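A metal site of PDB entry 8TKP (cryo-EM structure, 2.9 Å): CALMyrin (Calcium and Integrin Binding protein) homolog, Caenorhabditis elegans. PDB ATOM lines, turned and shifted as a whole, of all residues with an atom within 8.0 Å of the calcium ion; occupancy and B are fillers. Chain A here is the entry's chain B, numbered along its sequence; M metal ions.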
ATOM      1  N   LEU A 136     -17.602  21.911 -19.767  1.00  0.00           N
ATOM      2  CA  LEU A 136     -17.315  22.671 -18.570  1.00  0.00           C
ATOM      3  C   LEU A 136     -16.853  21.743 -17.463  1.00  0.00           C
ATOM      4  O   LEU A 136     -17.390  20.646 -17.295  1.00  0.00           O
ATOM      5  CB  LEU A 136     -18.540  23.490 -18.116  1.00  0.00           C
ATOM      6  CG  LEU A 136     -19.952  22.923 -18.288  1.00  0.00           C
ATOM      7  CD1 LEU A 136     -20.276  21.868 -17.240  1.00  0.00           C
ATOM      8  CD2 LEU A 136     -20.967  24.059 -18.240  1.00  0.00           C
ATOM      9  N   LEU A 137     -15.839  22.181 -16.709  1.00  0.00           N
ATOM     10  CA  LEU A 137     -15.300  21.389 -15.604  1.00  0.00           C
ATOM     11  C   LEU A 137     -16.251  21.490 -14.427  1.00  0.00           C
ATOM     12  O   LEU A 137     -16.275  22.499 -13.705  1.00  0.00           O
ATOM     13  CB  LEU A 137     -13.907  21.867 -15.231  1.00  0.00           C
ATOM     14  CG  LEU A 137     -12.857  21.900 -16.340  1.00  0.00           C
ATOM     15  CD1 LEU A 137     -11.503  22.314 -15.785  1.00  0.00           C
ATOM     16  CD2 LEU A 137     -12.764  20.566 -17.036  1.00  0.00           C
ATOM     17  N   ILE A 167     -13.656  26.612  -7.382  1.00  0.00           N
ATOM     18  CA  ILE A 167     -14.834  27.205  -8.014  1.00  0.00           C
ATOM     19  C   ILE A 167     -14.947  28.675  -7.649  1.00  0.00           C
ATOM     20  O   ILE A 167     -15.166  29.529  -8.505  1.00  0.00           O
ATOM     21  CB  ILE A 167     -16.095  26.416  -7.612  1.00  0.00           C
ATOM     22  CG1 ILE A 167     -16.075  25.023  -8.238  1.00  0.00           C
ATOM     23  CG2 ILE A 167     -17.342  27.168  -8.037  1.00  0.00           C
ATOM     24  CD1 ILE A 167     -17.274  24.182  -7.895  1.00  0.00           C
ATOM     25  N   ALA A 170     -12.428  30.669  -9.601  1.00  0.00           N
ATOM     26  CA  ALA A 170     -12.564  30.699 -11.052  1.00  0.00           C
ATOM     27  C   ALA A 170     -13.968  31.016 -11.539  1.00  0.00           C
ATOM     28  O   ALA A 170     -14.112  31.724 -12.542  1.00  0.00           O
ATOM     29  CB  ALA A 170     -12.126  29.357 -11.648  1.00  0.00           C
ATOM     30  N   ASP A 171     -15.010  30.528 -10.872  1.00  0.00           N
ATOM     31  CA  ASP A 171     -16.379  30.667 -11.357  1.00  0.00           C
ATOM     32  C   ASP A 171     -16.852  32.096 -11.112  1.00  0.00           C
ATOM     33  O   ASP A 171     -17.382  32.439 -10.049  1.00  0.00           O
ATOM     34  CB  ASP A 171     -17.283  29.644 -10.680  1.00  0.00           C
ATOM     35  CG  ASP A 171     -18.667  29.592 -11.301  1.00  0.00           C
ATOM     36  OD1 ASP A 171     -19.293  30.657 -11.481  1.00  0.00           O
ATOM     37  OD2 ASP A 171     -19.136  28.480 -11.603  1.00  0.00           O
ATOM     38  N   LEU A 172     -16.662  32.940 -12.117  1.00  0.00           N
ATOM     39  CA  LEU A 172     -17.164  34.302 -12.071  1.00  0.00           C
ATOM     40  C   LEU A 172     -18.539  34.456 -12.696  1.00  0.00           C
ATOM     41  O   LEU A 172     -19.095  35.563 -12.656  1.00  0.00           O
ATOM     42  CB  LEU A 172     -16.168  35.252 -12.756  1.00  0.00           C
ATOM     43  CG  LEU A 172     -15.549  34.810 -14.088  1.00  0.00           C
ATOM     44  CD1 LEU A 172     -16.473  35.093 -15.255  1.00  0.00           C
ATOM     45  CD2 LEU A 172     -14.201  35.485 -14.298  1.00  0.00           C
ATOM     46  N   ASP A 173     -19.106  33.399 -13.269  1.00  0.00           N
ATOM     47  CA  ASP A 173     -20.436  33.433 -13.851  1.00  0.00           C
ATOM     48  C   ASP A 173     -21.526  32.964 -12.905  1.00  0.00           C
ATOM     49  O   ASP A 173     -22.705  33.081 -13.228  1.00  0.00           O
ATOM     50  CB  ASP A 173     -20.478  32.592 -15.137  1.00  0.00           C
ATOM     51  CG  ASP A 173     -19.594  33.152 -16.225  1.00  0.00           C
ATOM     52  OD1 ASP A 173     -19.461  34.386 -16.317  1.00  0.00           O
ATOM     53  OD2 ASP A 173     -19.018  32.350 -16.991  1.00  0.00           O
ATOM     54  N   GLY A 174     -21.158  32.429 -11.735  1.00  0.00           N
ATOM     55  CA  GLY A 174     -22.152  31.900 -10.827  1.00  0.00           C
ATOM     56  C   GLY A 174     -22.850  30.656 -11.306  1.00  0.00           C
ATOM     57  O   GLY A 174     -23.949  30.346 -10.842  1.00  0.00           O
ATOM     58  N   ASP A 175     -22.248  29.925 -12.243  1.00  0.00           N
ATOM     59  CA  ASP A 175     -22.847  28.728 -12.813  1.00  0.00           C
ATOM     60  C   ASP A 175     -22.340  27.445 -12.170  1.00  0.00           C
ATOM     61  O   ASP A 175     -22.639  26.361 -12.671  1.00  0.00           O
ATOM     62  CB  ASP A 175     -22.591  28.679 -14.322  1.00  0.00           C
ATOM     63  CG  ASP A 175     -21.168  29.038 -14.686  1.00  0.00           C
ATOM     64  OD1 ASP A 175     -20.442  29.562 -13.814  1.00  0.00           O
ATOM     65  OD2 ASP A 175     -20.766  28.805 -15.841  1.00  0.00           O
ATOM     66  N   SER A 176     -21.578  27.538 -11.070  1.00  0.00           N
ATOM     67  CA  SER A 176     -21.081  26.370 -10.339  1.00  0.00           C
ATOM     68  C   SER A 176     -20.205  25.477 -11.202  1.00  0.00           C
ATOM     69  O   SER A 176     -20.064  24.284 -10.931  1.00  0.00           O
ATOM     70  CB  SER A 176     -22.237  25.561  -9.726  1.00  0.00           C
ATOM     71  OG  SER A 176     -23.003  26.357  -8.841  1.00  0.00           O
ATOM     72  N   SER A 177     -19.608  26.036 -12.251  1.00  0.00           N
ATOM     73  CA  SER A 177     -18.749  25.274 -13.147  1.00  0.00           C
ATOM     74  C   SER A 177     -17.811  26.235 -13.862  1.00  0.00           C
ATOM     75  O   SER A 177     -18.081  27.435 -13.953  1.00  0.00           O
ATOM     76  CB  SER A 177     -19.559  24.460 -14.154  1.00  0.00           C
ATOM     77  OG  SER A 177     -20.413  25.300 -14.910  1.00  0.00           O
ATOM     78  N   ILE A 178     -16.714  25.699 -14.361  1.00  0.00           N
ATOM     79  CA  ILE A 178     -15.664  26.478 -14.993  1.00  0.00           C
ATOM     80  C   ILE A 178     -15.779  26.280 -16.500  1.00  0.00           C
ATOM     81  O   ILE A 178     -15.433  25.214 -17.021  1.00  0.00           O
ATOM     82  CB  ILE A 178     -14.267  26.095 -14.485  1.00  0.00           C
ATOM     83  CG1 ILE A 178     -14.204  26.231 -12.967  1.00  0.00           C
ATOM     84  CG2 ILE A 178     -13.208  26.963 -15.138  1.00  0.00           C
ATOM     85  CD1 ILE A 178     -12.872  25.824 -12.377  1.00  0.00           C
ATOM     86  N   ASN A 179     -16.264  27.303 -17.199  1.00  0.00           N
ATOM     87  CA  ASN A 179     -16.215  27.295 -18.649  1.00  0.00           C
ATOM     88  C   ASN A 179     -14.769  27.479 -19.120  1.00  0.00           C
ATOM     89  O   ASN A 179     -13.881  27.827 -18.345  1.00  0.00           O
ATOM     90  CB  ASN A 179     -17.096  28.406 -19.230  1.00  0.00           C
ATOM     91  CG  ASN A 179     -18.552  28.250 -18.829  1.00  0.00           C
ATOM     92  OD1 ASN A 179     -19.019  27.138 -18.560  1.00  0.00           O
ATOM     93  ND2 ASN A 179     -19.269  29.359 -18.779  1.00  0.00           N
ATOM     94  N   PHE A 180     -14.550  27.249 -20.416  1.00  0.00           N
ATOM     95  CA  PHE A 180     -13.192  27.324 -20.935  1.00  0.00           C
ATOM     96  C   PHE A 180     -12.619  28.728 -20.839  1.00  0.00           C
ATOM     97  O   PHE A 180     -11.398  28.891 -20.720  1.00  0.00           O
ATOM     98  CB  PHE A 180     -13.125  26.842 -22.387  1.00  0.00           C
ATOM     99  CG  PHE A 180     -11.787  27.057 -23.019  1.00  0.00           C
ATOM    100  CD1 PHE A 180     -10.696  26.321 -22.594  1.00  0.00           C
ATOM    101  CD2 PHE A 180     -11.608  28.015 -23.996  1.00  0.00           C
ATOM    102  CE1 PHE A 180      -9.450  26.524 -23.156  1.00  0.00           C
ATOM    103  CE2 PHE A 180     -10.362  28.218 -24.557  1.00  0.00           C
ATOM    104  CZ  PHE A 180      -9.290  27.475 -24.133  1.00  0.00           C
ATOM    105  N   ALA A 181     -13.466  29.754 -20.898  1.00  0.00           N
ATOM    106  CA  ALA A 181     -12.965  31.122 -20.741  1.00  0.00           C
ATOM    107  C   ALA A 181     -12.415  31.354 -19.344  1.00  0.00           C
ATOM    108  O   ALA A 181     -11.315  31.899 -19.182  1.00  0.00           O
ATOM    109  CB  ALA A 181     -14.079  32.118 -21.060  1.00  0.00           C
ATOM    110  N   GLU A 182     -13.162  30.941 -18.318  1.00  0.00           N
ATOM    111  CA  GLU A 182     -12.685  31.082 -16.949  1.00  0.00           C
ATOM    112  C   GLU A 182     -11.413  30.261 -16.733  1.00  0.00           C
ATOM    113  O   GLU A 182     -10.463  30.726 -16.090  1.00  0.00           O
ATOM    114  CB  GLU A 182     -13.773  30.636 -15.973  1.00  0.00           C
ATOM    115  CG  GLU A 182     -15.075  31.426 -16.079  1.00  0.00           C
ATOM    116  CD  GLU A 182     -16.267  30.655 -15.547  1.00  0.00           C
ATOM    117  OE1 GLU A 182     -16.450  29.489 -15.937  1.00  0.00           O
ATOM    118  OE2 GLU A 182     -17.021  31.219 -14.728  1.00  0.00           O
ATOM    119  N   PHE A 183     -11.375  29.047 -17.272  1.00  0.00           N
ATOM    120  CA  PHE A 183     -10.200  28.199 -17.136  1.00  0.00           C
ATOM    121  C   PHE A 183      -8.977  28.829 -17.805  1.00  0.00           C
ATOM    122  O   PHE A 183      -7.887  28.865 -17.224  1.00  0.00           O
ATOM    123  CB  PHE A 183     -10.494  26.816 -17.722  1.00  0.00           C
ATOM    124  CG  PHE A 183      -9.310  25.884 -17.724  1.00  0.00           C
ATOM    125  CD1 PHE A 183      -9.025  25.113 -16.610  1.00  0.00           C
ATOM    126  CD2 PHE A 183      -8.498  25.785 -18.831  1.00  0.00           C
ATOM    127  CE1 PHE A 183      -7.941  24.250 -16.613  1.00  0.00           C
ATOM    128  CE2 PHE A 183      -7.418  24.930 -18.845  1.00  0.00           C
ATOM    129  CZ  PHE A 183      -7.145  24.166 -17.731  1.00  0.00           C
HETATM  130 CA    CA M   1     -18.591  29.423 -15.179  1.00  0.00          CA
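The calcium ion is bound by OE1 of Glu 182 (2.3 Å), OD1 of Asp 175 (2.3 Å), OD2 of Asp 175 (2.4 Å), O of Ser 177 (2.4 Å) and OE2 of Glu 182 (2.4 Å).
Residues that only touch the calcium ion: Asp 173 (3.5 Å), Asn 179 (3.7 Å) and Asp 171 (3.7 Å).
Within 4 Å of the calcium ion: Asp 171, Asp 173, Asp 175, Ser 177, Asn 179 and Glu 182.
Along chain A the residues within 4 Å of the calcium ion span positions 171 to 182.
The nearest printed residue that does not touch the calcium ion is Ile 178 (4.2 Å).
The backbone NH (N) of Ser 177 lies within hydrogen-bond range of the side-chain carboxylate (OD2) of Asp 171 (2.6 Å).
The side-chain carboxylate (OE2) of Glu 182 lies close to the backbone NH (N) of Leu 172, at 3.1 Å.
The side-chain carboxylate (OE2) of Glu 182 lies close to the backbone NH (N) of Asp 173 (3.4 Å).
The backbone NH (N) of Asn 179 lies close to the side-chain carboxylate (OE1) of Glu 182 (2.5 Å).
The side-chain carboxylate of Asp 171 lies within hydrogen-bond range of the backbone NH of Ser 176.
ND2 of Asn 179 lies within hydrogen-bond range of OD2 of Asp 173.
OD1 of Asp 171 sits at hydrogen-bond distance from N of Gly 174.
The side-chain carboxylate of Asp 171 sits at hydrogen-bond distance from the backbone NH of Asp 173, at 3.3 Å.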
